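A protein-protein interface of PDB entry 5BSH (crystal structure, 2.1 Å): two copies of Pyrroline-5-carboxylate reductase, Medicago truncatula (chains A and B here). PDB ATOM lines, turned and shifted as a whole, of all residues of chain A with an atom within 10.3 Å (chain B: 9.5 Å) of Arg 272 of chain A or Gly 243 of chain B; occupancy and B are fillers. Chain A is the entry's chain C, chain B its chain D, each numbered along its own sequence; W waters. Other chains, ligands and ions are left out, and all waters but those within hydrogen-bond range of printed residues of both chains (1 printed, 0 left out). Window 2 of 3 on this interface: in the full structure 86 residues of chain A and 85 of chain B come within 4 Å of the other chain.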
ATOM      1  N   GLY A 110      -4.816   9.449  -0.966  1.00  0.00           N
ATOM      2  CA  GLY A 110      -4.248   9.597  -2.307  1.00  0.00           C
ATOM      3  C   GLY A 110      -3.961   8.334  -3.100  1.00  0.00           C
ATOM      4  O   GLY A 110      -3.597   8.420  -4.250  1.00  0.00           O
ATOM      5  N   PHE A 175     -12.427  10.903  -5.528  1.00  0.00           N
ATOM      6  CA  PHE A 175     -11.674  11.002  -4.239  1.00  0.00           C
ATOM      7  C   PHE A 175     -10.779  12.283  -4.051  1.00  0.00           C
ATOM      8  O   PHE A 175     -10.686  12.855  -2.957  1.00  0.00           O
ATOM      9  CB  PHE A 175     -10.911   9.682  -3.947  1.00  0.00           C
ATOM     10  CG  PHE A 175     -11.768   8.638  -3.242  1.00  0.00           C
ATOM     11  CD1 PHE A 175     -12.966   8.231  -3.783  1.00  0.00           C
ATOM     12  CD2 PHE A 175     -11.422   8.152  -2.011  1.00  0.00           C
ATOM     13  CE1 PHE A 175     -13.798   7.316  -3.132  1.00  0.00           C
ATOM     14  CE2 PHE A 175     -12.224   7.227  -1.370  1.00  0.00           C
ATOM     15  CZ  PHE A 175     -13.408   6.792  -1.927  1.00  0.00           C
ATOM     16  N   ASP A 176     -10.222  12.827  -5.110  1.00  0.00           N
ATOM     17  CA  ASP A 176      -9.626  14.209  -5.016  1.00  0.00           C
ATOM     18  C   ASP A 176     -10.540  15.338  -4.595  1.00  0.00           C
ATOM     19  O   ASP A 176     -10.269  16.154  -3.707  1.00  0.00           O
ATOM     20  CB  ASP A 176      -9.157  14.643  -6.391  1.00  0.00           C
ATOM     21  CG  ASP A 176      -7.931  13.892  -6.827  1.00  0.00           C
ATOM     22  OD1 ASP A 176      -7.182  13.488  -5.913  1.00  0.00           O
ATOM     23  OD2 ASP A 176      -7.734  13.768  -8.073  1.00  0.00           O
ATOM     24  N   ALA A 177     -11.679  15.406  -5.224  1.00  0.00           N
ATOM     25  CA  ALA A 177     -12.655  16.356  -4.812  1.00  0.00           C
ATOM     26  C   ALA A 177     -13.195  16.103  -3.366  1.00  0.00           C
ATOM     27  O   ALA A 177     -13.515  17.054  -2.604  1.00  0.00           O
ATOM     28  CB  ALA A 177     -13.807  16.325  -5.790  1.00  0.00           C
ATOM     29  N   THR A 179     -11.587  14.914  -1.024  1.00  0.00           N
ATOM     30  CA  THR A 179     -10.508  15.352  -0.150  1.00  0.00           C
ATOM     31  C   THR A 179     -10.619  16.877   0.175  1.00  0.00           C
ATOM     32  O   THR A 179     -10.403  17.332   1.298  1.00  0.00           O
ATOM     33  CB  THR A 179      -9.117  14.966  -0.738  1.00  0.00           C
ATOM     34  OG1 THR A 179      -9.065  13.564  -0.878  1.00  0.00           O
ATOM     35  CG2 THR A 179      -7.952  15.395   0.150  1.00  0.00           C
ATOM     36  N   GLY A 180     -10.975  17.623  -0.825  1.00  0.00           N
ATOM     37  CA  GLY A 180     -11.085  19.083  -0.708  1.00  0.00           C
ATOM     38  C   GLY A 180     -12.265  19.464   0.166  1.00  0.00           C
ATOM     39  O   GLY A 180     -12.323  20.584   0.630  1.00  0.00           O
ATOM     40  N   LEU A 181     -13.249  18.579   0.247  1.00  0.00           N
ATOM     41  CA  LEU A 181     -14.512  18.880   0.934  1.00  0.00           C
ATOM     42  C   LEU A 181     -14.490  18.238   2.338  1.00  0.00           C
ATOM     43  O   LEU A 181     -14.349  18.936   3.319  1.00  0.00           O
ATOM     44  CB  LEU A 181     -15.694  18.431   0.100  1.00  0.00           C
ATOM     45  CG  LEU A 181     -17.092  18.556   0.725  1.00  0.00           C
ATOM     46  CD1 LEU A 181     -17.304  19.960   1.281  1.00  0.00           C
ATOM     47  CD2 LEU A 181     -18.187  18.241  -0.214  1.00  0.00           C
ATOM     48  N   SER A 184     -10.569  18.210   3.951  1.00  0.00           N
ATOM     49  CA  SER A 184     -10.014  19.516   4.311  1.00  0.00           C
ATOM     50  C   SER A 184     -10.981  20.417   4.981  1.00  0.00           C
ATOM     51  O   SER A 184     -10.609  21.327   5.676  1.00  0.00           O
ATOM     52  CB  SER A 184      -9.511  20.194   3.021  1.00  0.00           C
ATOM     53  OG  SER A 184      -8.532  19.401   2.415  1.00  0.00           O
ATOM     54  N   TYR A 188     -11.765  24.609   7.543  1.00  0.00           N
ATOM     55  CA  TYR A 188     -12.565  25.764   7.183  1.00  0.00           C
ATOM     56  C   TYR A 188     -13.493  26.090   8.330  1.00  0.00           C
ATOM     57  O   TYR A 188     -13.737  27.251   8.650  1.00  0.00           O
ATOM     58  CB  TYR A 188     -13.340  25.561   5.915  1.00  0.00           C
ATOM     59  CG  TYR A 188     -12.603  24.900   4.785  1.00  0.00           C
ATOM     60  CD1 TYR A 188     -11.219  24.929   4.687  1.00  0.00           C
ATOM     61  CD2 TYR A 188     -13.304  24.281   3.774  1.00  0.00           C
ATOM     62  CE1 TYR A 188     -10.544  24.321   3.605  1.00  0.00           C
ATOM     63  CE2 TYR A 188     -12.667  23.670   2.682  1.00  0.00           C
ATOM     64  CZ  TYR A 188     -11.276  23.647   2.641  1.00  0.00           C
ATOM     65  OH  TYR A 188     -10.650  22.966   1.592  1.00  0.00           O
ATOM     66  N   ASN A 264     -14.400  28.652  -3.422  1.00  0.00           N
ATOM     67  CA  ASN A 264     -13.007  28.731  -3.800  1.00  0.00           C
ATOM     68  C   ASN A 264     -12.098  27.788  -2.994  1.00  0.00           C
ATOM     69  O   ASN A 264     -11.142  27.271  -3.524  1.00  0.00           O
ATOM     70  CB  ASN A 264     -12.517  30.103  -3.618  1.00  0.00           C
ATOM     71  CG  ASN A 264     -13.152  31.116  -4.588  1.00  0.00           C
ATOM     72  OD1 ASN A 264     -13.694  30.766  -5.617  1.00  0.00           O
ATOM     73  ND2 ASN A 264     -12.948  32.343  -4.304  1.00  0.00           N
ATOM     74  N   ALA A 265     -12.375  27.669  -1.682  1.00  0.00           N
ATOM     75  CA  ALA A 265     -11.542  26.841  -0.878  1.00  0.00           C
ATOM     76  C   ALA A 265     -11.633  25.398  -1.299  1.00  0.00           C
ATOM     77  O   ALA A 265     -10.598  24.663  -1.422  1.00  0.00           O
ATOM     78  CB  ALA A 265     -11.897  26.983   0.583  1.00  0.00           C
ATOM     79  N   VAL A 266     -12.875  24.917  -1.451  1.00  0.00           N
ATOM     80  CA  VAL A 266     -13.083  23.515  -1.834  1.00  0.00           C
ATOM     81  C   VAL A 266     -12.445  23.247  -3.153  1.00  0.00           C
ATOM     82  O   VAL A 266     -11.664  22.260  -3.317  1.00  0.00           O
ATOM     83  CB  VAL A 266     -14.562  23.137  -1.949  1.00  0.00           C
ATOM     84  CG1 VAL A 266     -14.704  21.749  -2.494  1.00  0.00           C
ATOM     85  CG2 VAL A 266     -15.189  23.211  -0.581  1.00  0.00           C
ATOM     86  N   VAL A 267     -12.682  24.117  -4.126  1.00  0.00           N
ATOM     87  CA  VAL A 267     -12.019  23.968  -5.437  1.00  0.00           C
ATOM     88  C   VAL A 267     -10.456  23.952  -5.369  1.00  0.00           C
ATOM     89  O   VAL A 267      -9.823  23.161  -6.060  1.00  0.00           O
ATOM     90  CB  VAL A 267     -12.489  25.034  -6.412  1.00  0.00           C
ATOM     91  CG1 VAL A 267     -11.691  25.052  -7.742  1.00  0.00           C
ATOM     92  CG2 VAL A 267     -13.970  24.755  -6.723  1.00  0.00           C
ATOM     93  N   ALA A 268      -9.852  24.859  -4.620  1.00  0.00           N
ATOM     94  CA  ALA A 268      -8.424  24.937  -4.637  1.00  0.00           C
ATOM     95  C   ALA A 268      -7.859  23.683  -3.910  1.00  0.00           C
ATOM     96  O   ALA A 268      -6.841  23.128  -4.301  1.00  0.00           O
ATOM     97  CB  ALA A 268      -7.951  26.160  -3.906  1.00  0.00           C
ATOM     98  N   ALA A 269      -8.518  23.264  -2.840  1.00  0.00           N
ATOM     99  CA  ALA A 269      -8.079  22.089  -2.181  1.00  0.00           C
ATOM    100  C   ALA A 269      -8.172  20.850  -3.064  1.00  0.00           C
ATOM    101  O   ALA A 269      -7.284  19.968  -3.024  1.00  0.00           O
ATOM    102  CB  ALA A 269      -8.856  21.876  -0.908  1.00  0.00           C
ATOM    103  N   ALA A 270      -9.273  20.706  -3.746  1.00  0.00           N
ATOM    104  CA  ALA A 270      -9.441  19.595  -4.728  1.00  0.00           C
ATOM    105  C   ALA A 270      -8.387  19.635  -5.816  1.00  0.00           C
ATOM    106  O   ALA A 270      -7.813  18.593  -6.221  1.00  0.00           O
ATOM    107  CB  ALA A 270     -10.805  19.588  -5.377  1.00  0.00           C
ATOM    108  N   LYS A 271      -8.126  20.810  -6.309  1.00  0.00           N
ATOM    109  CA  LYS A 271      -7.059  20.927  -7.280  1.00  0.00           C
ATOM    110  C   LYS A 271      -5.675  20.501  -6.716  1.00  0.00           C
ATOM    111  O   LYS A 271      -4.880  19.868  -7.385  1.00  0.00           O
ATOM    112  CB  LYS A 271      -7.040  22.326  -7.813  1.00  0.00           C
ATOM    113  CG  LYS A 271      -5.892  22.572  -8.762  1.00  0.00           C
ATOM    114  CD  LYS A 271      -5.904  23.975  -9.338  1.00  0.00           C
ATOM    115  CE  LYS A 271      -4.662  24.163 -10.192  1.00  0.00           C
ATOM    116  NZ  LYS A 271      -4.420  25.606 -10.366  1.00  0.00           N
ATOM    117  N   ARG A 272      -5.384  20.883  -5.487  1.00  0.00           N
ATOM    118  CA  ARG A 272      -4.121  20.505  -4.879  1.00  0.00           C
ATOM    119  C   ARG A 272      -4.044  18.980  -4.686  1.00  0.00           C
ATOM    120  O   ARG A 272      -2.983  18.385  -4.852  1.00  0.00           O
ATOM    121  CB  ARG A 272      -3.910  21.221  -3.550  1.00  0.00           C
ATOM    122  CG  ARG A 272      -2.594  20.877  -2.889  1.00  0.00           C
ATOM    123  CD  ARG A 272      -1.394  21.226  -3.759  1.00  0.00           C
ATOM    124  NE  ARG A 272      -0.150  21.148  -2.979  1.00  0.00           N
ATOM    125  CZ  ARG A 272       1.061  20.900  -3.468  1.00  0.00           C
ATOM    126  NH1 ARG A 272       1.218  20.644  -4.762  1.00  0.00           N
ATOM    127  NH2 ARG A 272       2.116  20.886  -2.640  1.00  0.00           N
ATOM    128  N   SER A 273      -5.156  18.370  -4.340  1.00  0.00           N
ATOM    129  CA  SER A 273      -5.199  16.938  -4.114  1.00  0.00           C
ATOM    130  C   SER A 273      -4.873  16.264  -5.424  1.00  0.00           C
ATOM    131  O   SER A 273      -4.093  15.320  -5.501  1.00  0.00           O
ATOM    132  CB  SER A 273      -6.552  16.538  -3.647  1.00  0.00           C
ATOM    133  OG  SER A 273      -6.670  15.132  -3.627  1.00  0.00           O
ATOM    134  N   GLN A 274      -5.417  16.774  -6.492  1.00  0.00           N
ATOM    135  CA  GLN A 274      -5.137  16.194  -7.803  1.00  0.00           C
ATOM    136  C   GLN A 274      -3.651  16.353  -8.139  1.00  0.00           C
ATOM    137  O   GLN A 274      -3.032  15.434  -8.677  1.00  0.00           O
ATOM    138  CB  GLN A 274      -6.050  16.811  -8.878  1.00  0.00           C
ATOM    139  CG  GLN A 274      -5.963  16.194 -10.258  1.00  0.00           C
ATOM    140  CD  GLN A 274      -4.715  16.620 -10.992  1.00  0.00           C
ATOM    141  OE1 GLN A 274      -4.326  17.802 -10.969  1.00  0.00           O
ATOM    142  NE2 GLN A 274      -4.069  15.664 -11.658  1.00  0.00           N
ATOM    143  N   GLU A 275      -3.081  17.513  -7.848  1.00  0.00           N
ATOM    144  CA  GLU A 275      -1.685  17.751  -8.152  1.00  0.00           C
ATOM    145  C   GLU A 275      -0.753  16.864  -7.357  1.00  0.00           C
ATOM    146  O   GLU A 275       0.300  16.590  -7.798  1.00  0.00           O
ATOM    147  CB  GLU A 275      -1.288  19.176  -7.816  1.00  0.00           C
ATOM    148  CG  GLU A 275      -1.835  20.244  -8.709  1.00  0.00           C
ATOM    149  CD  GLU A 275      -1.539  21.637  -8.150  1.00  0.00           C
ATOM    150  OE1 GLU A 275      -0.783  21.786  -7.117  1.00  0.00           O
ATOM    151  OE2 GLU A 275      -2.011  22.558  -8.844  1.00  0.00           O
ATOM    152  N   LEU A 276      -1.144  16.497  -6.142  1.00  0.00           N
ATOM    153  CA  LEU A 276      -0.306  15.636  -5.292  1.00  0.00           C
ATOM    154  C   LEU A 276      -0.506  14.222  -5.747  1.00  0.00           C
ATOM    155  O   LEU A 276      -0.095  13.310  -5.133  1.00  0.00           O
ATOM    156  CB  LEU A 276      -0.671  15.804  -3.816  1.00  0.00           C
ATOM    157  CG  LEU A 276      -0.232  17.182  -3.286  1.00  0.00           C
ATOM    158  CD1 LEU A 276      -0.848  17.411  -1.918  1.00  0.00           C
ATOM    159  CD2 LEU A 276       1.296  17.282  -3.224  1.00  0.00           C
ATOM    160  N   SER A 277      -1.270  14.120  -6.814  1.00  0.00           N
ATOM    161  CA  SER A 277      -1.311  13.063  -7.840  1.00  0.00           C
ATOM    162  C   SER A 277      -2.675  12.447  -7.636  1.00  0.00           C
ATOM    163  O   SER A 277      -2.987  12.073  -6.519  1.00  0.00           O
ATOM    164  CB  SER A 277      -0.183  12.024  -7.822  1.00  0.00           C
ATOM    165  OG  SER A 277      -0.781  10.741  -7.845  1.00  0.00           O
ATOM    166  OXT SER A 277      -3.489  12.380  -8.554  1.00  0.00           O
ATOM    167  N   ALA B 203     -16.307  21.131  -8.062  1.00  0.00           N
ATOM    168  CA  ALA B 203     -15.106  20.257  -8.272  1.00  0.00           C
ATOM    169  C   ALA B 203     -15.421  18.900  -8.835  1.00  0.00           C
ATOM    170  O   ALA B 203     -14.573  18.012  -8.839  1.00  0.00           O
ATOM    171  CB  ALA B 203     -14.365  20.108  -6.945  1.00  0.00           C
ATOM    172  N   VAL B 239      -4.747  19.598  11.236  1.00  0.00           N
ATOM    173  CA  VAL B 239      -5.159  19.040   9.950  1.00  0.00           C
ATOM    174  C   VAL B 239      -4.425  19.632   8.763  1.00  0.00           C
ATOM    175  O   VAL B 239      -4.665  19.255   7.643  1.00  0.00           O
ATOM    176  CB  VAL B 239      -6.702  19.111   9.722  1.00  0.00           C
ATOM    177  CG1 VAL B 239      -7.412  18.259  10.760  1.00  0.00           C
ATOM    178  CG2 VAL B 239      -7.242  20.516   9.835  1.00  0.00           C
ATOM    179  N   THR B 240      -3.615  20.654   8.988  1.00  0.00           N
ATOM    180  CA  THR B 240      -2.959  21.339   7.869  1.00  0.00           C
ATOM    181  C   THR B 240      -1.550  20.737   7.577  1.00  0.00           C
ATOM    182  O   THR B 240      -0.550  21.297   7.979  1.00  0.00           O
ATOM    183  CB  THR B 240      -2.883  22.850   8.076  1.00  0.00           C
ATOM    184  OG1 THR B 240      -2.585  23.191   9.420  1.00  0.00           O
ATOM    185  CG2 THR B 240      -4.290  23.513   7.800  1.00  0.00           C
ATOM    186  N   SER B 241      -1.518  19.633   6.833  1.00  0.00           N
ATOM    187  CA  SER B 241      -0.294  18.982   6.413  1.00  0.00           C
ATOM    188  C   SER B 241       0.528  19.904   5.543  1.00  0.00           C
ATOM    189  O   SER B 241      -0.017  20.646   4.736  1.00  0.00           O
ATOM    190  CB  SER B 241      -0.563  17.775   5.493  1.00  0.00           C
ATOM    191  OG  SER B 241      -1.593  17.041   6.021  1.00  0.00           O
ATOM    192  N   PRO B 242       1.827  19.773   5.611  1.00  0.00           N
ATOM    193  CA  PRO B 242       2.747  20.655   4.861  1.00  0.00           C
ATOM    194  C   PRO B 242       2.488  20.661   3.380  1.00  0.00           C
ATOM    195  O   PRO B 242       2.442  19.629   2.783  1.00  0.00           O
ATOM    196  CB  PRO B 242       4.142  20.018   5.123  1.00  0.00           C
ATOM    197  CG  PRO B 242       3.983  19.337   6.438  1.00  0.00           C
ATOM    198  CD  PRO B 242       2.538  18.895   6.568  1.00  0.00           C
ATOM    199  N   GLY B 243       2.251  21.836   2.802  1.00  0.00           N
ATOM    200  CA  GLY B 243       1.999  21.949   1.330  1.00  0.00           C
ATOM    201  C   GLY B 243       0.789  21.159   0.823  1.00  0.00           C
ATOM    202  O   GLY B 243       0.673  20.896  -0.350  1.00  0.00           O
ATOM    203  N   GLY B 244      -0.096  20.762   1.731  1.00  0.00           N
ATOM    204  CA  GLY B 244      -1.172  19.869   1.388  1.00  0.00           C
ATOM    205  C   GLY B 244      -2.481  20.588   0.962  1.00  0.00           C
ATOM    206  O   GLY B 244      -2.521  21.795   0.750  1.00  0.00           O
ATOM    207  N   THR B 245      -3.517  19.779   0.831  1.00  0.00           N
ATOM    208  CA  THR B 245      -4.782  20.193   0.329  1.00  0.00           C
ATOM    209  C   THR B 245      -5.468  21.136   1.270  1.00  0.00           C
ATOM    210  O   THR B 245      -6.002  22.159   0.859  1.00  0.00           O
ATOM    211  CB  THR B 245      -5.698  18.964   0.032  1.00  0.00           C
ATOM    212  OG1 THR B 245      -6.061  18.334   1.243  1.00  0.00           O
ATOM    213  CG2 THR B 245      -5.036  17.970  -0.874  1.00  0.00           C
ATOM    214  N   THR B 246      -5.391  20.832   2.555  1.00  0.00           N
ATOM    215  CA  THR B 246      -6.059  21.626   3.576  1.00  0.00           C
ATOM    216  C   THR B 246      -5.567  23.032   3.677  1.00  0.00           C
ATOM    217  O   THR B 246      -6.371  24.045   3.611  1.00  0.00           O
ATOM    218  CB  THR B 246      -6.081  20.900   4.905  1.00  0.00           C
ATOM    219  OG1 THR B 246      -6.613  19.579   4.705  1.00  0.00           O
ATOM    220  CG2 THR B 246      -6.954  21.597   5.849  1.00  0.00           C
ATOM    221  N   ILE B 247      -4.273  23.180   3.730  1.00  0.00           N
ATOM    222  CA  ILE B 247      -3.672  24.522   3.742  1.00  0.00           C
ATOM    223  C   ILE B 247      -3.935  25.310   2.469  1.00  0.00           C
ATOM    224  O   ILE B 247      -4.016  26.544   2.485  1.00  0.00           O
ATOM    225  CB  ILE B 247      -2.152  24.488   4.080  1.00  0.00           C
ATOM    226  CG1 ILE B 247      -1.645  25.900   4.472  1.00  0.00           C
ATOM    227  CG2 ILE B 247      -1.289  23.970   2.948  1.00  0.00           C
ATOM    228  CD1 ILE B 247      -2.201  26.344   5.785  1.00  0.00           C
ATOM    229  N   ALA B 248      -4.005  24.639   1.311  1.00  0.00           N
ATOM    230  CA  ALA B 248      -4.327  25.357   0.081  1.00  0.00           C
ATOM    231  C   ALA B 248      -5.742  25.956   0.196  1.00  0.00           C
ATOM    232  O   ALA B 248      -6.001  27.078  -0.180  1.00  0.00           O
ATOM    233  CB  ALA B 248      -4.249  24.410  -1.140  1.00  0.00           C
ATOM    234  N   GLY B 249      -6.660  25.218   0.769  1.00  0.00           N
ATOM    235  CA  GLY B 249      -7.998  25.715   0.979  1.00  0.00           C
ATOM    236  C   GLY B 249      -8.042  26.797   2.030  1.00  0.00           C
ATOM    237  O   GLY B 249      -8.669  27.894   1.814  1.00  0.00           O
ATOM    238  N   VAL B 250      -7.341  26.589   3.113  1.00  0.00           N
ATOM    239  CA  VAL B 250      -7.272  27.628   4.146  1.00  0.00           C
ATOM    240  C   VAL B 250      -6.675  28.926   3.595  1.00  0.00           C
ATOM    241  O   VAL B 250      -7.178  30.033   3.886  1.00  0.00           O
ATOM    242  CB  VAL B 250      -6.511  27.145   5.354  1.00  0.00           C
ATOM    243  CG1 VAL B 250      -6.148  28.270   6.260  1.00  0.00           C
ATOM    244  CG2 VAL B 250      -7.369  26.133   6.105  1.00  0.00           C
ATOM    245  N   GLU B 252      -6.986  30.170   0.630  1.00  0.00           N
ATOM    246  CA  GLU B 252      -8.043  30.911  -0.138  1.00  0.00           C
ATOM    247  C   GLU B 252      -8.953  31.604   0.806  1.00  0.00           C
ATOM    248  O   GLU B 252      -9.366  32.739   0.556  1.00  0.00           O
ATOM    249  CB  GLU B 252      -8.862  29.998  -1.036  1.00  0.00           C
ATOM    250  CG  GLU B 252      -8.080  29.411  -2.190  1.00  0.00           C
ATOM    251  CD  GLU B 252      -7.582  30.495  -3.159  1.00  0.00           C
ATOM    252  OE1 GLU B 252      -8.435  31.334  -3.478  1.00  0.00           O
ATOM    253  OE2 GLU B 252      -6.379  30.492  -3.405  1.00  0.00           O
HETATM  254  O   HOH W   1     -10.552  33.131  -2.004  1.00  0.00           O
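The side-chain hydroxyl (OG1) of Thr 245 of chain B sits at hydrogen-bond distance from the side-chain hydroxyl (OG) of Ser 184 of chain A.
The backbone carbonyl oxygen of Gly 243 of chain B is in hydrogen-bond range of the guanidinium group of Arg 272 of chain A (2.7 Å).
The side-chain hydroxyl of Ser 184 of chain A sits at hydrogen-bond distance from the side-chain hydroxyl of Thr 246 of chain B (3.0 Å).
The backbone carbonyl oxygen of Gly 180 of chain A lies within hydrogen-bond range of the side-chain hydroxyl of Tyr 188 of chain A (3.1 Å).
OG of Ser 273 of chain A lies within hydrogen-bond range of OD1 of Asp 176 of chain A, at 2.9 Å.
The side-chain hydroxyl of Tyr 188 of chain A lies within hydrogen-bond range of the backbone carbonyl oxygen of Ala 265 of chain A (3.5 Å).
The guanidinium group (NH1) of Arg 272 of chain A is in salt-bridge range of the side-chain carboxylate (OE1) of Glu 275 of chain A (3.3 Å).
The backbone NH of Ser 184 of chain A is in hydrogen-bond range of the backbone carbonyl oxygen of Thr 179 of chain A, 2.8 Å away.
The side-chain hydroxyl (OG1) of Thr 179 of chain A sits at hydrogen-bond distance from the backbone carbonyl oxygen (O) of Phe 175 of chain A (2.7 Å).
Ala 203 of chain B touches Ala 177 of chain A.
CG2 of Thr 179 of chain A touches OG1 of Thr 245 of chain B (3.7 Å).
C of Gly 249 of chain B touches CE1 of Tyr 188 of chain A, 3.9 Å away.
Tyr 188 of chain A touches Val 250 of chain B.
Asn 264 of chain A touches Glu 252 of chain B.
CB of Ala 265 of chain A touches O of Gly 249 of chain B, at 3.6 Å.
Ala 268 of chain A touches Glu 252 of chain B.
Arg 272 of chain A touches Gly 244 of chain B (CG to O, 3.8 Å).
CG of Arg 272 of chain A touches CA of Thr 245 of chain B (3.95 Å).
Thr 245 of chain B touches Ser 273 of chain A (CG2 to CA, 3.4 Å).
Asp 176 of chain A touches none of the printed residues of chain B.
Of the printed residues of chain B, Thr 179 of chain A touches Thr 245 (3.7 Å).
Printed residues of chain B within 4 Å of Ala 269 of chain A: Thr 245 (3.4 Å).
Of the printed residues of chain B, Arg 272 of chain A touches Gly 243, Gly 244 and Thr 245.
Of chain B, only Thr 245 (3.4 Å) comes within 4 Å of Ser 273 of chain A.
No residue of chain B comes within 4 Å of Glu 275 of chain A.
Of the printed residues of chain A, Gly 243 of chain B touches Arg 272.
Of the printed residues of chain A, Gly 244 of chain B touches Arg 272.
Ile 247 of chain B touches none of the printed residues of chain A.
The nearest printed residue of chain B that does not touch Arg 272 of chain A is Ala 248 of chain B (4.01 Å).
Of the 23 printed residues of chain A, 11 touch a printed residue of chain B.
Hydrophobic or aromatic side chains of chain A that line the printed part of chain B: Ala 177, Tyr 188, Ala 265, Ala 268, Ala 269 and Ala 270.
Hydrophobic or aromatic side chains of chain B that line the printed part of chain A: Ala 203.
Among the printed residues, 15 pairs touch across the chains.
Among the printed residues, no Asp or Glu carboxylate lies within 4 Å of a Lys or Arg side-chain nitrogen of the other chain.
No position is printed for both chains.
Of the 15 pairs that touch across the chains among the printed residues, none has its exchanged pair printed and touching as well.
Water W1 bridges O of Glu 252 of chain B (2.8 Å) and ND2 of Asn 264 of chain A (3.4 Å).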
